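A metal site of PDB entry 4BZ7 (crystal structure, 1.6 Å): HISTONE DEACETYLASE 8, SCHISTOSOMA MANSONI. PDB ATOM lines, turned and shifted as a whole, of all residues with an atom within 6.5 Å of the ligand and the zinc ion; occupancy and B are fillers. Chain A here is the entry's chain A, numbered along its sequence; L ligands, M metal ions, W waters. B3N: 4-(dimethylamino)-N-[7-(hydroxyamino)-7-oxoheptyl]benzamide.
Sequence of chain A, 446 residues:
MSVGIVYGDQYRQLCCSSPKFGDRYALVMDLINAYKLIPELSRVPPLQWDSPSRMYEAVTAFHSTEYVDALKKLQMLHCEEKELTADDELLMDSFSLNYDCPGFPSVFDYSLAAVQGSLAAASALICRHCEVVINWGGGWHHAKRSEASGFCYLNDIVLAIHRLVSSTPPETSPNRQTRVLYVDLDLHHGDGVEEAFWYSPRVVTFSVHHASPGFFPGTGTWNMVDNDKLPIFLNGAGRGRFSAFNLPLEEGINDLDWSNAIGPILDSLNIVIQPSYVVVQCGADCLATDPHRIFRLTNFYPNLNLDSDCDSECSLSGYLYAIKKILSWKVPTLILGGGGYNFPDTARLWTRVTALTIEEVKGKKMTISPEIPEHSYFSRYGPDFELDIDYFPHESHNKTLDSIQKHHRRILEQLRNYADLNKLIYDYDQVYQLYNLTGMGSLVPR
OH of Tyr 341 lies close to O2 of the ligand (2.5 Å). A ring nitrogen (NE2) of His 142 is in hydrogen-bond range of a nitrogen (N3) of the ligand, 2.6 Å away. A ring nitrogen (NE2) of His 141 is in hydrogen-bond range of a nitrogen (N3) of the ligand, 3.4 Å away. The side-chain carboxylate (OD2) of Asp 100 is in hydrogen-bond range of a nitrogen (N12) of the ligand (3.0 Å).
The backbone NH (N) of Leu 187 sits at hydrogen-bond distance from the side-chain carboxylate (OD1) of Asp 285. The side-chain carboxylate (OD2) of Asp 186 lies within hydrogen-bond range of the backbone NH (N) of Gly 339, 3.0 Å away. The side-chain carboxylate (OD2) of Asp 186 lies within hydrogen-bond range of the side-chain amide nitrogen (NE2) of Gln 281 (3.1 Å). A ring nitrogen (NE2) of His 142 lies within hydrogen-bond range of a ring nitrogen (NE2) of His 141. The side-chain sulfur of Cys 152 lies within hydrogen-bond range of the backbone NH of His 142, at 3.6 Å. O of Gly 150 is in hydrogen-bond range of SG of Cys 152 (3.5 Å).
Tyr 99 touches the ligand (CD1 to C22, 3.6 Å). Gly 150 touches the ligand (O to C5, 3.7 Å). CE2 of Phe 151 touches C5 of the ligand (3.7 Å). CD2 of Phe 216 touches C7 of the ligand, 3.6 Å away. Hydrophobic or aromatic side chains within 4 Å of the ligand: Tyr 99, His 141, His 142, Phe 151, His 188, Phe 216 and Tyr 341. Within 4 Å of the ligand: Tyr 99, Asp 100, His 141, His 142, Gly 150, Phe 151, Asp 186, His 188, Phe 216, Asp 285 and Tyr 341. The nearest printed residue that does not touch the ligand is Gly 339 (4.2 Å).
Of the 23 residues printed, 3 come within 4 Å of the zinc ion. The nearest printed residue that does not touch the zinc ion is Gly 339 (4.2 Å).
OD2 of Asp 285 binds the zinc ion (1.9 Å). The zinc ion is bound by OD1 of Asp 186. The zinc ion is bound by ND1 of His 188, at 2.0 Å. The zinc ion is bound by O4 of the ligand (2.1 Å). O2 of the ligand binds the zinc ion. The zinc ion has five donor atoms within binding distance.
Water W1 lies within hydrogen-bond range of NE2 of His 141 (3.2 Å), N3 of the ligand (3.3 Å) and N of Gly 339 (3.3 Å). Water W2 bridges the backbone carbonyl oxygen (O) of Gly 150 (2.9 Å) and the side-chain hydroxyl (OH) of Tyr 341 (3.2 Å).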
ATOM      1  N   PHE A  21      -2.896  24.525 -25.887  1.00  0.00           N
ATOM      2  CA  PHE A  21      -2.463  25.007 -24.559  1.00  0.00           C
ATOM      3  C   PHE A  21      -0.979  24.983 -24.286  1.00  0.00           C
ATOM      4  O   PHE A  21      -0.543  25.547 -23.290  1.00  0.00           O
ATOM      5  CB  PHE A  21      -3.280  24.330 -23.454  1.00  0.00           C
ATOM      6  CG  PHE A  21      -4.722  24.739 -23.514  1.00  0.00           C
ATOM      7  CD1 PHE A  21      -5.134  26.000 -23.104  1.00  0.00           C
ATOM      8  CD2 PHE A  21      -5.677  23.895 -24.079  1.00  0.00           C
ATOM      9  CE1 PHE A  21      -6.476  26.374 -23.174  1.00  0.00           C
ATOM     10  CE2 PHE A  21      -7.012  24.285 -24.173  1.00  0.00           C
ATOM     11  CZ  PHE A  21      -7.407  25.526 -23.730  1.00  0.00           C
ATOM     12  N   TYR A  99     -11.279  19.824 -37.193  1.00  0.00           N
ATOM     13  CA  TYR A  99     -11.275  21.276 -37.147  1.00  0.00           C
ATOM     14  C   TYR A  99     -10.591  21.829 -35.880  1.00  0.00           C
ATOM     15  O   TYR A  99      -9.382  21.608 -35.722  1.00  0.00           O
ATOM     16  CB  TYR A  99     -12.707  21.826 -37.386  1.00  0.00           C
ATOM     17  CG  TYR A  99     -13.324  21.318 -38.678  1.00  0.00           C
ATOM     18  CD1 TYR A  99     -12.730  21.599 -39.905  1.00  0.00           C
ATOM     19  CD2 TYR A  99     -14.475  20.546 -38.673  1.00  0.00           C
ATOM     20  CE1 TYR A  99     -13.289  21.147 -41.108  1.00  0.00           C
ATOM     21  CE2 TYR A  99     -15.018  20.047 -39.866  1.00  0.00           C
ATOM     22  CZ  TYR A  99     -14.418  20.354 -41.078  1.00  0.00           C
ATOM     23  OH  TYR A  99     -14.955  19.900 -42.271  1.00  0.00           O
ATOM     24  N   ASP A 100     -11.343  22.467 -34.959  1.00  0.00           N
ATOM     25  CA  ASP A 100     -10.779  23.017 -33.710  1.00  0.00           C
ATOM     26  C   ASP A 100     -10.482  21.991 -32.577  1.00  0.00           C
ATOM     27  O   ASP A 100      -9.871  22.343 -31.565  1.00  0.00           O
ATOM     28  CB  ASP A 100     -11.554  24.263 -33.204  1.00  0.00           C
ATOM     29  CG  ASP A 100     -11.309  25.539 -33.994  1.00  0.00           C
ATOM     30  OD1 ASP A 100     -10.478  25.508 -34.949  1.00  0.00           O
ATOM     31  OD2 ASP A 100     -11.940  26.570 -33.683  1.00  0.00           O
ATOM     32  N   GLY A 139     -10.751  20.948 -15.981  1.00  0.00           N
ATOM     33  CA  GLY A 139     -11.813  21.942 -16.240  1.00  0.00           C
ATOM     34  C   GLY A 139     -12.311  21.990 -17.675  1.00  0.00           C
ATOM     35  O   GLY A 139     -12.843  23.013 -18.109  1.00  0.00           O
ATOM     36  N   HIS A 141     -14.929  21.707 -19.760  1.00  0.00           N
ATOM     37  CA  HIS A 141     -16.370  21.721 -19.638  1.00  0.00           C
ATOM     38  C   HIS A 141     -17.240  21.444 -20.859  1.00  0.00           C
ATOM     39  O   HIS A 141     -18.419  21.178 -20.683  1.00  0.00           O
ATOM     40  CB  HIS A 141     -16.827  23.009 -18.912  1.00  0.00           C
ATOM     41  CG  HIS A 141     -16.483  24.315 -19.595  1.00  0.00           C
ATOM     42  ND1 HIS A 141     -17.019  25.506 -19.144  1.00  0.00           N
ATOM     43  CD2 HIS A 141     -15.627  24.587 -20.609  1.00  0.00           C
ATOM     44  CE1 HIS A 141     -16.521  26.458 -19.909  1.00  0.00           C
ATOM     45  NE2 HIS A 141     -15.668  25.960 -20.807  1.00  0.00           N
ATOM     46  N   HIS A 142     -16.673  21.517 -22.057  1.00  0.00           N
ATOM     47  CA  HIS A 142     -17.478  21.358 -23.271  1.00  0.00           C
ATOM     48  C   HIS A 142     -17.640  19.935 -23.798  1.00  0.00           C
ATOM     49  O   HIS A 142     -18.502  19.725 -24.655  1.00  0.00           O
ATOM     50  CB  HIS A 142     -16.893  22.209 -24.403  1.00  0.00           C
ATOM     51  CG  HIS A 142     -16.849  23.677 -24.096  1.00  0.00           C
ATOM     52  ND1 HIS A 142     -18.011  24.392 -23.797  1.00  0.00           N
ATOM     53  CD2 HIS A 142     -15.808  24.549 -24.124  1.00  0.00           C
ATOM     54  CE1 HIS A 142     -17.627  25.653 -23.621  1.00  0.00           C
ATOM     55  NE2 HIS A 142     -16.304  25.797 -23.822  1.00  0.00           N
ATOM     56  N   SER A 149     -15.517  19.016 -28.202  1.00  0.00           N
ATOM     57  CA  SER A 149     -16.044  20.366 -28.436  1.00  0.00           C
ATOM     58  C   SER A 149     -15.168  21.407 -27.750  1.00  0.00           C
ATOM     59  O   SER A 149     -14.705  21.148 -26.629  1.00  0.00           O
ATOM     60  CB  SER A 149     -17.459  20.472 -27.853  1.00  0.00           C
ATOM     61  OG  SER A 149     -17.973  21.789 -28.014  1.00  0.00           O
ATOM     62  N   GLY A 150     -14.892  22.518 -28.418  1.00  0.00           N
ATOM     63  CA  GLY A 150     -14.166  23.632 -27.789  1.00  0.00           C
ATOM     64  C   GLY A 150     -12.853  23.286 -27.133  1.00  0.00           C
ATOM     65  O   GLY A 150     -12.576  23.732 -26.010  1.00  0.00           O
ATOM     66  N   PHE A 151     -12.044  22.494 -27.837  1.00  0.00           N
ATOM     67  CA  PHE A 151     -10.711  22.040 -27.399  1.00  0.00           C
ATOM     68  C   PHE A 151     -10.790  21.058 -26.219  1.00  0.00           C
ATOM     69  O   PHE A 151      -9.754  20.765 -25.616  1.00  0.00           O
ATOM     70  CB  PHE A 151      -9.759  23.238 -27.095  1.00  0.00           C
ATOM     71  CG  PHE A 151      -9.951  24.553 -27.868  1.00  0.00           C
ATOM     72  CD1 PHE A 151      -9.972  24.559 -29.267  1.00  0.00           C
ATOM     73  CD2 PHE A 151     -10.065  25.761 -27.203  1.00  0.00           C
ATOM     74  CE1 PHE A 151     -10.155  25.751 -29.973  1.00  0.00           C
ATOM     75  CE2 PHE A 151     -10.226  26.968 -27.918  1.00  0.00           C
ATOM     76  CZ  PHE A 151     -10.271  26.955 -29.294  1.00  0.00           C
ATOM     77  N   CYS A 152     -11.996  20.525 -25.921  1.00  0.00           N
ATOM     78  CA  CYS A 152     -12.256  19.569 -24.823  1.00  0.00           C
ATOM     79  C   CYS A 152     -12.517  18.212 -25.427  1.00  0.00           C
ATOM     80  O   CYS A 152     -13.458  18.094 -26.232  1.00  0.00           O
ATOM     81  CB  CYS A 152     -13.457  20.003 -23.976  1.00  0.00           C
ATOM     82  SG  CYS A 152     -13.261  21.649 -23.235  1.00  0.00           S
ATOM     83  N   ASP A 186     -15.898  30.412 -16.326  1.00  0.00           N
ATOM     84  CA  ASP A 186     -15.265  30.601 -17.616  1.00  0.00           C
ATOM     85  C   ASP A 186     -16.068  31.605 -18.466  1.00  0.00           C
ATOM     86  O   ASP A 186     -17.277  31.780 -18.266  1.00  0.00           O
ATOM     87  CB  ASP A 186     -15.274  29.246 -18.353  1.00  0.00           C
ATOM     88  CG  ASP A 186     -14.342  29.128 -19.534  1.00  0.00           C
ATOM     89  OD1 ASP A 186     -14.725  29.584 -20.630  1.00  0.00           O
ATOM     90  OD2 ASP A 186     -13.247  28.575 -19.371  1.00  0.00           O
ATOM     91  N   LEU A 187     -15.395  32.271 -19.402  1.00  0.00           N
ATOM     92  CA  LEU A 187     -16.053  33.193 -20.325  1.00  0.00           C
ATOM     93  C   LEU A 187     -17.179  32.494 -21.120  1.00  0.00           C
ATOM     94  O   LEU A 187     -18.168  33.148 -21.487  1.00  0.00           O
ATOM     95  CB  LEU A 187     -15.005  33.715 -21.325  1.00  0.00           C
ATOM     96  CG  LEU A 187     -15.490  34.735 -22.372  1.00  0.00           C
ATOM     97  CD1 LEU A 187     -15.971  36.048 -21.714  1.00  0.00           C
ATOM     98  CD2 LEU A 187     -14.364  35.041 -23.336  1.00  0.00           C
ATOM     99  N   HIS A 188     -16.995  31.201 -21.382  1.00  0.00           N
ATOM    100  CA  HIS A 188     -17.937  30.393 -22.165  1.00  0.00           C
ATOM    101  C   HIS A 188     -18.918  29.621 -21.319  1.00  0.00           C
ATOM    102  O   HIS A 188     -18.599  29.178 -20.203  1.00  0.00           O
ATOM    103  CB  HIS A 188     -17.174  29.437 -23.103  1.00  0.00           C
ATOM    104  CG  HIS A 188     -16.236  30.164 -24.026  1.00  0.00           C
ATOM    105  ND1 HIS A 188     -14.935  30.430 -23.648  1.00  0.00           N
ATOM    106  CD2 HIS A 188     -16.473  30.709 -25.245  1.00  0.00           C
ATOM    107  CE1 HIS A 188     -14.386  31.066 -24.687  1.00  0.00           C
ATOM    108  NE2 HIS A 188     -15.288  31.260 -25.665  1.00  0.00           N
ATOM    109  N   HIS A 189     -20.115  29.430 -21.888  1.00  0.00           N
ATOM    110  CA  HIS A 189     -21.153  28.614 -21.232  1.00  0.00           C
ATOM    111  C   HIS A 189     -20.624  27.173 -21.011  1.00  0.00           C
ATOM    112  O   HIS A 189     -20.116  26.553 -21.933  1.00  0.00           O
ATOM    113  CB  HIS A 189     -22.385  28.554 -22.119  1.00  0.00           C
ATOM    114  CG  HIS A 189     -23.476  27.690 -21.550  1.00  0.00           C
ATOM    115  ND1 HIS A 189     -24.108  26.725 -22.332  1.00  0.00           N
ATOM    116  CD2 HIS A 189     -23.988  27.638 -20.288  1.00  0.00           C
ATOM    117  CE1 HIS A 189     -25.005  26.149 -21.529  1.00  0.00           C
ATOM    118  NE2 HIS A 189     -24.978  26.682 -20.296  1.00  0.00           N
ATOM    119  N   PHE A 216     -19.479  31.247 -29.338  1.00  0.00           N
ATOM    120  CA  PHE A 216     -19.450  29.868 -28.912  1.00  0.00           C
ATOM    121  C   PHE A 216     -19.865  29.698 -27.425  1.00  0.00           C
ATOM    122  O   PHE A 216     -19.421  30.494 -26.594  1.00  0.00           O
ATOM    123  CB  PHE A 216     -18.004  29.379 -29.062  1.00  0.00           C
ATOM    124  CG  PHE A 216     -17.837  27.910 -28.741  1.00  0.00           C
ATOM    125  CD1 PHE A 216     -18.103  26.928 -29.697  1.00  0.00           C
ATOM    126  CD2 PHE A 216     -17.497  27.488 -27.452  1.00  0.00           C
ATOM    127  CE1 PHE A 216     -17.961  25.574 -29.402  1.00  0.00           C
ATOM    128  CE2 PHE A 216     -17.337  26.136 -27.155  1.00  0.00           C
ATOM    129  CZ  PHE A 216     -17.595  25.189 -28.121  1.00  0.00           C
ATOM    130  N   GLN A 281     -15.268  25.727 -11.884  1.00  0.00           N
ATOM    131  CA  GLN A 281     -14.432  25.801 -13.072  1.00  0.00           C
ATOM    132  C   GLN A 281     -13.995  27.264 -13.111  1.00  0.00           C
ATOM    133  O   GLN A 281     -14.830  28.169 -13.081  1.00  0.00           O
ATOM    134  CB  GLN A 281     -15.242  25.359 -14.309  1.00  0.00           C
ATOM    135  CG  GLN A 281     -14.365  25.035 -15.529  1.00  0.00           C
ATOM    136  CD  GLN A 281     -14.116  26.247 -16.407  1.00  0.00           C
ATOM    137  OE1 GLN A 281     -14.266  27.398 -15.993  1.00  0.00           O
ATOM    138  NE2 GLN A 281     -13.778  25.987 -17.670  1.00  0.00           N
ATOM    139  N   GLY A 283     -11.960  29.012 -15.476  1.00  0.00           N
ATOM    140  CA  GLY A 283     -11.350  29.398 -16.758  1.00  0.00           C
ATOM    141  C   GLY A 283     -10.992  30.867 -16.735  1.00  0.00           C
ATOM    142  O   GLY A 283     -11.800  31.679 -16.285  1.00  0.00           O
ATOM    143  N   ASP A 285     -10.338  33.048 -19.117  1.00  0.00           N
ATOM    144  CA  ASP A 285     -10.606  33.822 -20.341  1.00  0.00           C
ATOM    145  C   ASP A 285     -11.505  35.048 -20.164  1.00  0.00           C
ATOM    146  O   ASP A 285     -11.761  35.782 -21.132  1.00  0.00           O
ATOM    147  CB  ASP A 285     -11.034  32.908 -21.520  1.00  0.00           C
ATOM    148  CG  ASP A 285     -12.021  31.816 -21.184  1.00  0.00           C
ATOM    149  OD1 ASP A 285     -12.519  31.811 -20.041  1.00  0.00           O
ATOM    150  OD2 ASP A 285     -12.306  30.968 -22.093  1.00  0.00           O
ATOM    151  N   HIS A 292      -9.451  36.979 -26.188  1.00  0.00           N
ATOM    152  CA  HIS A 292     -10.882  37.094 -26.562  1.00  0.00           C
ATOM    153  C   HIS A 292     -11.315  38.544 -26.452  1.00  0.00           C
ATOM    154  O   HIS A 292     -12.181  38.998 -27.220  1.00  0.00           O
ATOM    155  CB  HIS A 292     -11.770  36.262 -25.645  1.00  0.00           C
ATOM    156  CG  HIS A 292     -11.836  34.823 -26.034  1.00  0.00           C
ATOM    157  ND1 HIS A 292     -10.966  33.884 -25.492  1.00  0.00           N
ATOM    158  CD2 HIS A 292     -12.675  34.191 -26.895  1.00  0.00           C
ATOM    159  CE1 HIS A 292     -11.323  32.725 -26.021  1.00  0.00           C
ATOM    160  NE2 HIS A 292     -12.320  32.856 -26.887  1.00  0.00           N
ATOM    161  N   GLY A 338      -9.418  25.605 -16.940  1.00  0.00           N
ATOM    162  CA  GLY A 338     -10.295  25.713 -18.107  1.00  0.00           C
ATOM    163  C   GLY A 338      -9.677  26.606 -19.141  1.00  0.00           C
ATOM    164  O   GLY A 338      -8.471  26.512 -19.397  1.00  0.00           O
ATOM    165  N   GLY A 339     -10.470  27.485 -19.754  1.00  0.00           N
ATOM    166  CA  GLY A 339      -9.931  28.388 -20.769  1.00  0.00           C
ATOM    167  C   GLY A 339      -8.912  29.351 -20.199  1.00  0.00           C
ATOM    168  O   GLY A 339      -8.741  29.468 -18.994  1.00  0.00           O
ATOM    169  N   GLY A 340      -8.203  30.021 -21.101  1.00  0.00           N
ATOM    170  CA  GLY A 340      -7.223  31.019 -20.671  1.00  0.00           C
ATOM    171  C   GLY A 340      -6.123  30.966 -21.682  1.00  0.00           C
ATOM    172  O   GLY A 340      -5.274  30.065 -21.643  1.00  0.00           O
ATOM    173  N   TYR A 341      -6.139  31.914 -22.599  1.00  0.00           N
ATOM    174  CA  TYR A 341      -5.296  31.952 -23.762  1.00  0.00           C
ATOM    175  C   TYR A 341      -4.132  32.922 -23.711  1.00  0.00           C
ATOM    176  O   TYR A 341      -3.291  32.922 -24.603  1.00  0.00           O
ATOM    177  CB  TYR A 341      -6.207  32.082 -25.007  1.00  0.00           C
ATOM    178  CG  TYR A 341      -7.282  31.007 -24.956  1.00  0.00           C
ATOM    179  CD1 TYR A 341      -7.007  29.705 -25.354  1.00  0.00           C
ATOM    180  CD2 TYR A 341      -8.515  31.257 -24.341  1.00  0.00           C
ATOM    181  CE1 TYR A 341      -7.959  28.696 -25.234  1.00  0.00           C
ATOM    182  CE2 TYR A 341      -9.468  30.244 -24.207  1.00  0.00           C
ATOM    183  CZ  TYR A 341      -9.170  28.961 -24.627  1.00  0.00           C
ATOM    184  OH  TYR A 341     -10.099  27.950 -24.498  1.00  0.00           O
HETATM  185  O23 B3N L   1     -16.997  27.206 -33.809  1.00  0.00           O
HETATM  186  C13 B3N L   1     -15.883  27.104 -34.210  1.00  0.00           C
HETATM  187  C14 B3N L   1     -15.648  26.528 -35.559  1.00  0.00           C
HETATM  188  C15 B3N L   1     -14.299  26.592 -36.133  1.00  0.00           C
HETATM  189  C16 B3N L   1     -14.069  26.076 -37.412  1.00  0.00           C
HETATM  190  C17 B3N L   1     -15.117  25.435 -38.152  1.00  0.00           C
HETATM  191  N20 B3N L   1     -14.877  24.898 -39.488  1.00  0.00           N
HETATM  192  C22 B3N L   1     -13.623  25.105 -40.159  1.00  0.00           C
HETATM  193  C21 B3N L   1     -15.892  24.088 -40.160  1.00  0.00           C
HETATM  194  C18 B3N L   1     -16.443  25.385 -37.587  1.00  0.00           C
HETATM  195  C19 B3N L   1     -16.668  25.875 -36.271  1.00  0.00           C
HETATM  196  N12 B3N L   1     -14.751  27.568 -33.391  1.00  0.00           N
HETATM  197  C10 B3N L   1     -14.966  28.160 -32.080  1.00  0.00           C
HETATM  198  C9  B3N L   1     -14.361  27.360 -30.930  1.00  0.00           C
HETATM  199  C8  B3N L   1     -14.064  28.152 -29.652  1.00  0.00           C
HETATM  200  C7  B3N L   1     -14.017  27.353 -28.374  1.00  0.00           C
HETATM  201  C6  B3N L   1     -13.926  28.136 -27.042  1.00  0.00           C
HETATM  202  C5  B3N L   1     -13.262  27.347 -25.906  1.00  0.00           C
HETATM  203  C1  B3N L   1     -13.288  27.875 -24.487  1.00  0.00           C
HETATM  204  O2  B3N L   1     -12.468  28.721 -24.067  1.00  0.00           O
HETATM  205  N3  B3N L   1     -14.223  27.323 -23.598  1.00  0.00           N
HETATM  206  O4  B3N L   1     -14.267  27.662 -22.380  1.00  0.00           O
HETATM  207 ZN    ZN M   1     -13.688  29.632 -22.292  1.00  0.00          ZN
HETATM  208  O   HOH W   1     -12.554  25.565 -21.404  1.00  0.00           O
HETATM  209  O   HOH W   2     -11.374  25.104 -23.785  1.00  0.00           O
